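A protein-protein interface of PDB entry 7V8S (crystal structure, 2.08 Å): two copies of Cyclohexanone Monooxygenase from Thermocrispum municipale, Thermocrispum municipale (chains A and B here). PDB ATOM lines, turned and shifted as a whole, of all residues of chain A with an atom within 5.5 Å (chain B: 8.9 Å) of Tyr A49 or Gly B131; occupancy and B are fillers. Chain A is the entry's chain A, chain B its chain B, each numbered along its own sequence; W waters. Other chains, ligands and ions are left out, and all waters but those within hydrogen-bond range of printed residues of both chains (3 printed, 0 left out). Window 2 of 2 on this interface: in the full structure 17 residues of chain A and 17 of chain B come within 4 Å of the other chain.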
ATOM      1  N   GLY A  41     -16.240  20.280   2.875  1.00  0.00           N
ATOM      2  CA  GLY A  41     -17.283  21.287   2.612  1.00  0.00           C
ATOM      3  C   GLY A  41     -18.567  20.655   2.111  1.00  0.00           C
ATOM      4  O   GLY A  41     -18.483  19.559   1.531  1.00  0.00           O
ATOM      5  N   GLY A  42     -19.706  21.335   2.311  1.00  0.00           N
ATOM      6  CA  GLY A  42     -21.048  20.862   1.910  1.00  0.00           C
ATOM      7  C   GLY A  42     -21.324  21.086   0.433  1.00  0.00           C
ATOM      8  O   GLY A  42     -22.377  20.619  -0.048  1.00  0.00           O
ATOM      9  N   GLY A  43     -20.407  21.761  -0.265  1.00  0.00           N
ATOM     10  CA  GLY A  43     -20.433  21.944  -1.727  1.00  0.00           C
ATOM     11  C   GLY A  43     -19.029  22.097  -2.298  1.00  0.00           C
ATOM     12  O   GLY A  43     -18.091  22.325  -1.519  1.00  0.00           O
ATOM     13  N   VAL A  44     -18.899  21.934  -3.616  1.00  0.00           N
ATOM     14  CA  VAL A  44     -17.650  22.186  -4.392  1.00  0.00           C
ATOM     15  C   VAL A  44     -17.385  23.691  -4.362  1.00  0.00           C
ATOM     16  O   VAL A  44     -18.340  24.463  -4.054  1.00  0.00           O
ATOM     17  CB  VAL A  44     -17.755  21.657  -5.840  1.00  0.00           C
ATOM     18  CG1 VAL A  44     -18.081  20.165  -5.874  1.00  0.00           C
ATOM     19  CG2 VAL A  44     -18.771  22.427  -6.670  1.00  0.00           C
ATOM     20  N   GLY A  45     -16.146  24.080  -4.665  1.00  0.00           N
ATOM     21  CA  GLY A  45     -15.767  25.470  -4.979  1.00  0.00           C
ATOM     22  C   GLY A  45     -14.620  25.972  -4.116  1.00  0.00           C
ATOM     23  O   GLY A  45     -14.034  27.012  -4.472  1.00  0.00           O
ATOM     24  N   GLY A  46     -14.313  25.272  -3.019  1.00  0.00           N
ATOM     25  CA  GLY A  46     -13.267  25.670  -2.064  1.00  0.00           C
ATOM     26  C   GLY A  46     -13.515  27.080  -1.579  1.00  0.00           C
ATOM     27  O   GLY A  46     -14.623  27.327  -1.064  1.00  0.00           O
ATOM     28  N   THR A  47     -12.545  27.980  -1.774  1.00  0.00           N
ATOM     29  CA  THR A  47     -12.651  29.442  -1.520  1.00  0.00           C
ATOM     30  C   THR A  47     -14.073  29.941  -1.793  1.00  0.00           C
ATOM     31  O   THR A  47     -14.632  30.654  -0.967  1.00  0.00           O
ATOM     32  CB  THR A  47     -11.705  30.218  -2.445  1.00  0.00           C
ATOM     33  OG1 THR A  47     -10.385  29.705  -2.272  1.00  0.00           O
ATOM     34  CG2 THR A  47     -11.719  31.712  -2.202  1.00  0.00           C
ATOM     35  N   TRP A  48     -14.617  29.591  -2.952  1.00  0.00           N
ATOM     36  CA  TRP A  48     -15.850  30.194  -3.520  1.00  0.00           C
ATOM     37  C   TRP A  48     -17.106  29.523  -2.955  1.00  0.00           C
ATOM     38  O   TRP A  48     -18.210  30.042  -3.215  1.00  0.00           O
ATOM     39  CB  TRP A  48     -15.730  30.159  -5.039  1.00  0.00           C
ATOM     40  CG  TRP A  48     -14.460  30.838  -5.447  1.00  0.00           C
ATOM     41  CD1 TRP A  48     -13.310  30.266  -5.910  1.00  0.00           C
ATOM     42  CD2 TRP A  48     -14.170  32.234  -5.266  1.00  0.00           C
ATOM     43  NE1 TRP A  48     -12.348  31.222  -6.094  1.00  0.00           N
ATOM     44  CE2 TRP A  48     -12.843  32.438  -5.700  1.00  0.00           C
ATOM     45  CE3 TRP A  48     -14.908  33.325  -4.786  1.00  0.00           C
ATOM     46  CZ2 TRP A  48     -12.252  33.703  -5.684  1.00  0.00           C
ATOM     47  CZ3 TRP A  48     -14.326  34.576  -4.781  1.00  0.00           C
ATOM     48  CH2 TRP A  48     -13.012  34.757  -5.220  1.00  0.00           C
ATOM     49  N   TYR A  49     -16.933  28.461  -2.156  1.00  0.00           N
ATOM     50  CA  TYR A  49     -18.000  27.849  -1.322  1.00  0.00           C
ATOM     51  C   TYR A  49     -18.001  28.530   0.047  1.00  0.00           C
ATOM     52  O   TYR A  49     -19.063  29.006   0.469  1.00  0.00           O
ATOM     53  CB  TYR A  49     -17.812  26.340  -1.161  1.00  0.00           C
ATOM     54  CG  TYR A  49     -18.737  25.733  -0.135  1.00  0.00           C
ATOM     55  CD1 TYR A  49     -20.080  25.544  -0.413  1.00  0.00           C
ATOM     56  CD2 TYR A  49     -18.291  25.423   1.138  1.00  0.00           C
ATOM     57  CE1 TYR A  49     -20.947  25.010   0.531  1.00  0.00           C
ATOM     58  CE2 TYR A  49     -19.145  24.912   2.100  1.00  0.00           C
ATOM     59  CZ  TYR A  49     -20.478  24.694   1.792  1.00  0.00           C
ATOM     60  OH  TYR A  49     -21.329  24.180   2.726  1.00  0.00           O
ATOM     61  N   TRP A  50     -16.836  28.582   0.699  1.00  0.00           N
ATOM     62  CA  TRP A  50     -16.685  28.985   2.125  1.00  0.00           C
ATOM     63  C   TRP A  50     -16.921  30.499   2.302  1.00  0.00           C
ATOM     64  O   TRP A  50     -17.647  30.879   3.251  1.00  0.00           O
ATOM     65  CB  TRP A  50     -15.315  28.552   2.667  1.00  0.00           C
ATOM     66  CG  TRP A  50     -15.082  27.072   2.749  1.00  0.00           C
ATOM     67  CD1 TRP A  50     -14.242  26.334   1.963  1.00  0.00           C
ATOM     68  CD2 TRP A  50     -15.647  26.149   3.697  1.00  0.00           C
ATOM     69  NE1 TRP A  50     -14.269  25.017   2.338  1.00  0.00           N
ATOM     70  CE2 TRP A  50     -15.117  24.874   3.403  1.00  0.00           C
ATOM     71  CE3 TRP A  50     -16.556  26.266   4.755  1.00  0.00           C
ATOM     72  CZ2 TRP A  50     -15.463  23.736   4.130  1.00  0.00           C
ATOM     73  CZ3 TRP A  50     -16.892  25.142   5.480  1.00  0.00           C
ATOM     74  CH2 TRP A  50     -16.352  23.894   5.168  1.00  0.00           C
ATOM     75  N   ASN A  51     -16.346  31.343   1.436  1.00  0.00           N
ATOM     76  CA  ASN A  51     -16.320  32.820   1.630  1.00  0.00           C
ATOM     77  C   ASN A  51     -17.627  33.444   1.118  1.00  0.00           C
ATOM     78  O   ASN A  51     -17.606  34.062   0.037  1.00  0.00           O
ATOM     79  CB  ASN A  51     -15.078  33.438   0.988  1.00  0.00           C
ATOM     80  CG  ASN A  51     -13.823  33.045   1.738  1.00  0.00           C
ATOM     81  OD1 ASN A  51     -13.487  33.652   2.755  1.00  0.00           O
ATOM     82  ND2 ASN A  51     -13.171  31.987   1.280  1.00  0.00           N
ATOM     83  N   LYS A  52     -18.704  33.329   1.898  1.00  0.00           N
ATOM     84  CA  LYS A  52     -20.077  33.771   1.520  1.00  0.00           C
ATOM     85  C   LYS A  52     -20.323  35.218   1.974  1.00  0.00           C
ATOM     86  O   LYS A  52     -21.442  35.711   1.774  1.00  0.00           O
ATOM     87  CB  LYS A  52     -21.128  32.836   2.131  1.00  0.00           C
ATOM     88  CG  LYS A  52     -21.198  31.442   1.520  1.00  0.00           C
ATOM     89  CD  LYS A  52     -22.325  30.618   2.082  1.00  0.00           C
ATOM     90  CE  LYS A  52     -22.751  29.484   1.178  1.00  0.00           C
ATOM     91  NZ  LYS A  52     -21.794  28.358   1.247  1.00  0.00           N
ATOM     92  N   GLN A  86     -18.257  36.299  -5.616  1.00  0.00           N
ATOM     93  CA  GLN A  86     -18.134  34.906  -5.113  1.00  0.00           C
ATOM     94  C   GLN A  86     -19.251  34.028  -5.677  1.00  0.00           C
ATOM     95  O   GLN A  86     -18.973  32.914  -6.126  1.00  0.00           O
ATOM     96  CB  GLN A  86     -18.086  34.887  -3.590  1.00  0.00           C
ATOM     97  CG  GLN A  86     -18.368  33.523  -2.983  1.00  0.00           C
ATOM     98  CD  GLN A  86     -19.819  33.289  -2.649  1.00  0.00           C
ATOM     99  OE1 GLN A  86     -20.583  34.212  -2.356  1.00  0.00           O
ATOM    100  NE2 GLN A  86     -20.204  32.029  -2.665  1.00  0.00           N
ATOM    101  N   LEU A  90     -18.475  30.641  -7.963  1.00  0.00           N
ATOM    102  CA  LEU A  90     -19.030  29.353  -7.470  1.00  0.00           C
ATOM    103  C   LEU A  90     -19.874  28.711  -8.577  1.00  0.00           C
ATOM    104  O   LEU A  90     -19.709  27.507  -8.819  1.00  0.00           O
ATOM    105  CB  LEU A  90     -19.842  29.595  -6.198  1.00  0.00           C
ATOM    106  CG  LEU A  90     -20.500  28.360  -5.594  1.00  0.00           C
ATOM    107  CD1 LEU A  90     -19.452  27.388  -5.064  1.00  0.00           C
ATOM    108  CD2 LEU A  90     -21.479  28.766  -4.494  1.00  0.00           C
ATOM    109  N   GLN B 107     -28.645  12.695   4.934  1.00  0.00           N
ATOM    110  CA  GLN B 107     -27.362  13.269   4.456  1.00  0.00           C
ATOM    111  C   GLN B 107     -26.223  12.691   5.301  1.00  0.00           C
ATOM    112  O   GLN B 107     -26.121  13.042   6.491  1.00  0.00           O
ATOM    113  CB  GLN B 107     -27.429  14.796   4.518  1.00  0.00           C
ATOM    114  CG  GLN B 107     -26.188  15.468   3.949  1.00  0.00           C
ATOM    115  CD  GLN B 107     -26.404  16.952   3.784  1.00  0.00           C
ATOM    116  OE1 GLN B 107     -27.394  17.385   3.205  1.00  0.00           O
ATOM    117  NE2 GLN B 107     -25.476  17.742   4.296  1.00  0.00           N
ATOM    118  N   THR B 110     -22.212  14.126   7.626  1.00  0.00           N
ATOM    119  CA  THR B 110     -22.639  15.495   8.005  1.00  0.00           C
ATOM    120  C   THR B 110     -22.820  15.569   9.524  1.00  0.00           C
ATOM    121  O   THR B 110     -23.856  15.084  10.054  1.00  0.00           O
ATOM    122  CB  THR B 110     -23.856  15.943   7.190  1.00  0.00           C
ATOM    123  OG1 THR B 110     -23.499  15.863   5.810  1.00  0.00           O
ATOM    124  CG2 THR B 110     -24.286  17.353   7.523  1.00  0.00           C
ATOM    125  N   GLU B 111     -21.819  16.143  10.190  1.00  0.00           N
ATOM    126  CA  GLU B 111     -21.844  16.443  11.637  1.00  0.00           C
ATOM    127  C   GLU B 111     -22.562  17.774  11.847  1.00  0.00           C
ATOM    128  O   GLU B 111     -22.188  18.773  11.180  1.00  0.00           O
ATOM    129  CB  GLU B 111     -20.434  16.509  12.215  1.00  0.00           C
ATOM    130  CG  GLU B 111     -20.447  16.496  13.727  1.00  0.00           C
ATOM    131  CD  GLU B 111     -19.086  16.627  14.381  1.00  0.00           C
ATOM    132  OE1 GLU B 111     -18.108  16.886  13.663  1.00  0.00           O
ATOM    133  OE2 GLU B 111     -19.024  16.475  15.611  1.00  0.00           O
ATOM    134  N   VAL B 112     -23.562  17.790  12.727  1.00  0.00           N
ATOM    135  CA  VAL B 112     -24.166  19.059  13.221  1.00  0.00           C
ATOM    136  C   VAL B 112     -23.271  19.557  14.354  1.00  0.00           C
ATOM    137  O   VAL B 112     -23.033  18.777  15.288  1.00  0.00           O
ATOM    138  CB  VAL B 112     -25.627  18.881  13.662  1.00  0.00           C
ATOM    139  CG1 VAL B 112     -26.183  20.171  14.256  1.00  0.00           C
ATOM    140  CG2 VAL B 112     -26.483  18.400  12.504  1.00  0.00           C
ATOM    141  N   THR B 113     -22.720  20.762  14.203  1.00  0.00           N
ATOM    142  CA  THR B 113     -21.768  21.385  15.158  1.00  0.00           C
ATOM    143  C   THR B 113     -22.528  22.370  16.053  1.00  0.00           C
ATOM    144  O   THR B 113     -22.110  22.545  17.210  1.00  0.00           O
ATOM    145  CB  THR B 113     -20.610  22.066  14.417  1.00  0.00           C
ATOM    146  OG1 THR B 113     -21.157  23.017  13.506  1.00  0.00           O
ATOM    147  CG2 THR B 113     -19.754  21.092  13.634  1.00  0.00           C
ATOM    148  N   ASP B 114     -23.593  22.982  15.523  1.00  0.00           N
ATOM    149  CA  ASP B 114     -24.393  24.032  16.198  1.00  0.00           C
ATOM    150  C   ASP B 114     -25.880  23.761  15.981  1.00  0.00           C
ATOM    151  O   ASP B 114     -26.266  23.462  14.828  1.00  0.00           O
ATOM    152  CB  ASP B 114     -24.102  25.424  15.637  1.00  0.00           C
ATOM    153  CG  ASP B 114     -22.631  25.748  15.531  1.00  0.00           C
ATOM    154  OD1 ASP B 114     -21.950  25.099  14.714  1.00  0.00           O
ATOM    155  OD2 ASP B 114     -22.178  26.615  16.284  1.00  0.00           O
ATOM    156  N   VAL B 126     -29.586  25.404  12.408  1.00  0.00           N
ATOM    157  CA  VAL B 126     -28.664  24.234  12.487  1.00  0.00           C
ATOM    158  C   VAL B 126     -27.480  24.478  11.550  1.00  0.00           C
ATOM    159  O   VAL B 126     -27.710  24.803  10.374  1.00  0.00           O
ATOM    160  CB  VAL B 126     -29.414  22.929  12.162  1.00  0.00           C
ATOM    161  CG1 VAL B 126     -28.478  21.789  11.804  1.00  0.00           C
ATOM    162  CG2 VAL B 126     -30.325  22.531  13.315  1.00  0.00           C
ATOM    163  N   THR B 127     -26.256  24.344  12.066  1.00  0.00           N
ATOM    164  CA  THR B 127     -25.016  24.495  11.264  1.00  0.00           C
ATOM    165  C   THR B 127     -24.287  23.155  11.239  1.00  0.00           C
ATOM    166  O   THR B 127     -24.229  22.488  12.291  1.00  0.00           O
ATOM    167  CB  THR B 127     -24.136  25.639  11.777  1.00  0.00           C
ATOM    168  OG1 THR B 127     -24.933  26.823  11.735  1.00  0.00           O
ATOM    169  CG2 THR B 127     -22.875  25.822  10.960  1.00  0.00           C
ATOM    170  N   THR B 128     -23.766  22.787  10.070  1.00  0.00           N
ATOM    171  CA  THR B 128     -22.979  21.545   9.859  1.00  0.00           C
ATOM    172  C   THR B 128     -21.489  21.878   9.789  1.00  0.00           C
ATOM    173  O   THR B 128     -21.151  23.020   9.465  1.00  0.00           O
ATOM    174  CB  THR B 128     -23.417  20.827   8.581  1.00  0.00           C
ATOM    175  OG1 THR B 128     -22.942  21.614   7.485  1.00  0.00           O
ATOM    176  CG2 THR B 128     -24.916  20.625   8.514  1.00  0.00           C
ATOM    177  N   ALA B 129     -20.637  20.883  10.034  1.00  0.00           N
ATOM    178  CA  ALA B 129     -19.176  20.967   9.839  1.00  0.00           C
ATOM    179  C   ALA B 129     -18.897  21.384   8.387  1.00  0.00           C
ATOM    180  O   ALA B 129     -17.899  22.073   8.162  1.00  0.00           O
ATOM    181  CB  ALA B 129     -18.530  19.643  10.190  1.00  0.00           C
ATOM    182  N   GLY B 130     -19.757  20.993   7.437  1.00  0.00           N
ATOM    183  CA  GLY B 130     -19.582  21.302   6.002  1.00  0.00           C
ATOM    184  C   GLY B 130     -19.968  22.727   5.623  1.00  0.00           C
ATOM    185  O   GLY B 130     -19.861  23.044   4.422  1.00  0.00           O
ATOM    186  N   GLY B 131     -20.399  23.550   6.587  1.00  0.00           N
ATOM    187  CA  GLY B 131     -20.716  24.985   6.406  1.00  0.00           C
ATOM    188  C   GLY B 131     -22.111  25.229   5.835  1.00  0.00           C
ATOM    189  O   GLY B 131     -22.311  26.279   5.171  1.00  0.00           O
ATOM    190  N   GLU B 132     -23.053  24.309   6.065  1.00  0.00           N
ATOM    191  CA  GLU B 132     -24.492  24.514   5.756  1.00  0.00           C
ATOM    192  C   GLU B 132     -25.188  25.072   6.996  1.00  0.00           C
ATOM    193  O   GLU B 132     -24.908  24.568   8.100  1.00  0.00           O
ATOM    194  CB  GLU B 132     -25.178  23.221   5.323  1.00  0.00           C
ATOM    195  CG  GLU B 132     -24.935  22.882   3.868  1.00  0.00           C
ATOM    196  CD  GLU B 132     -25.670  21.640   3.410  1.00  0.00           C
ATOM    197  OE1 GLU B 132     -25.131  20.527   3.578  1.00  0.00           O
ATOM    198  OE2 GLU B 132     -26.791  21.798   2.906  1.00  0.00           O
ATOM    199  N   THR B 133     -26.039  26.081   6.801  1.00  0.00           N
ATOM    200  CA  THR B 133     -26.981  26.622   7.810  1.00  0.00           C
ATOM    201  C   THR B 133     -28.401  26.494   7.262  1.00  0.00           C
ATOM    202  O   THR B 133     -28.665  27.049   6.190  1.00  0.00           O
ATOM    203  CB  THR B 133     -26.674  28.081   8.148  1.00  0.00           C
ATOM    204  OG1 THR B 133     -25.329  28.122   8.616  1.00  0.00           O
ATOM    205  CG2 THR B 133     -27.605  28.641   9.198  1.00  0.00           C
ATOM    206  N   LEU B 134     -29.257  25.760   7.966  1.00  0.00           N
ATOM    207  CA  LEU B 134     -30.675  25.529   7.600  1.00  0.00           C
ATOM    208  C   LEU B 134     -31.508  25.811   8.846  1.00  0.00           C
ATOM    209  O   LEU B 134     -30.974  25.616   9.954  1.00  0.00           O
ATOM    210  CB  LEU B 134     -30.878  24.077   7.155  1.00  0.00           C
ATOM    211  CG  LEU B 134     -30.145  23.637   5.887  1.00  0.00           C
ATOM    212  CD1 LEU B 134     -30.419  22.171   5.616  1.00  0.00           C
ATOM    213  CD2 LEU B 134     -30.558  24.481   4.686  1.00  0.00           C
HETATM  214  O   HOH W   1     -24.004  19.067   1.720  1.00  0.00           O
HETATM  215  O   HOH W   2     -20.996  27.861   3.867  1.00  0.00           O
HETATM  216  O   HOH W   3     -23.468  26.248   2.334  1.00  0.00           O
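Water W2 bridges the backbone carbonyl oxygen (O) of Gly B131 and the side-chain amino group (NZ) of Lys A52.
Water W1 lies within hydrogen-bond range of the side-chain carboxylate (OE1) of Glu B132, the backbone carbonyl oxygen (O) of Gly A42 and the side-chain amide nitrogen (NE2) of Gln B107.
Water W3 lies within hydrogen-bond range of NZ of Lys A52 (2.9 Å), OH of Tyr A49 (3.0 Å) and O of Gly B131 (3.1 Å).
The backbone NH of Gly A42 is in hydrogen-bond range of the backbone carbonyl oxygen of Gly B130 (2.7 Å).
The side-chain hydroxyl (OH) of Tyr A49 lies within hydrogen-bond range of the backbone carbonyl oxygen (O) of Gly B130 (2.5 Å).
The side-chain hydroxyl (OH) of Tyr A49 sits at hydrogen-bond distance from the backbone carbonyl oxygen (O) of Gly B131, 3.4 Å away.
N of Gly A42 sits at hydrogen-bond distance from OH of Tyr A49 (3.3 Å).
The side-chain amino group (NZ) of Lys A52 lies within hydrogen-bond range of the backbone carbonyl oxygen (O) of Tyr A49 (2.9 Å).
The side-chain carboxylate of Glu B132 is in hydrogen-bond range of the side-chain amide nitrogen of Gln B107 (2.9 Å).
O of Glu B111 sits at hydrogen-bond distance from N of Ala B129 (2.9 Å).
N of Gly B130 lies close to OG1 of Thr B128, 3.2 Å away.
The backbone NH (N) of Glu B132 lies within hydrogen-bond range of the side-chain hydroxyl (OG1) of Thr B128 (3.0 Å).
Of the 15 printed residues of chain B, 4 touch a printed residue of chain A.
Along chain A the printed residues that touch a printed residue of chain B span positions 41 to 50.
Among the printed residues, 8 pairs touch across the chains.
Gly B131 touches just these residues of chain A: Tyr A49 and Trp A50.
Gly A42 touches just one residue of chain B: Gly B130 (2.7 Å).
No residue of chain B comes within 4 Å of Gly A45.
No residue of chain B comes within 4 Å of Gly A46.
Printed residues of chain A within 4 Å of Glu B132: Tyr A49.
Printed residues of chain B within 4 Å of Gly A41: Gly B130.
Printed residues of chain A within 4 Å of Ala B129: Trp A50.
Asn A51 touches none of the printed residues of chain B.
The nearest residue of chain B that does not touch Tyr A49 is Thr B128 (5.6 Å).
The nearest residue of chain A that does not touch Gly B131 is Lys A52 (4.5 Å).
The nearest printed residue of chain A that does not touch Gly B130 is Gly A43 (4.9 Å).
No position is printed for both chains.
Among the printed residues, pairs that only touch across the chains: Gly A41 with Gly B130, Tyr A49 with Glu B132, Trp A50 with Ala B129, Trp A50 with Gly B130 and Trp A50 with Gly B131.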
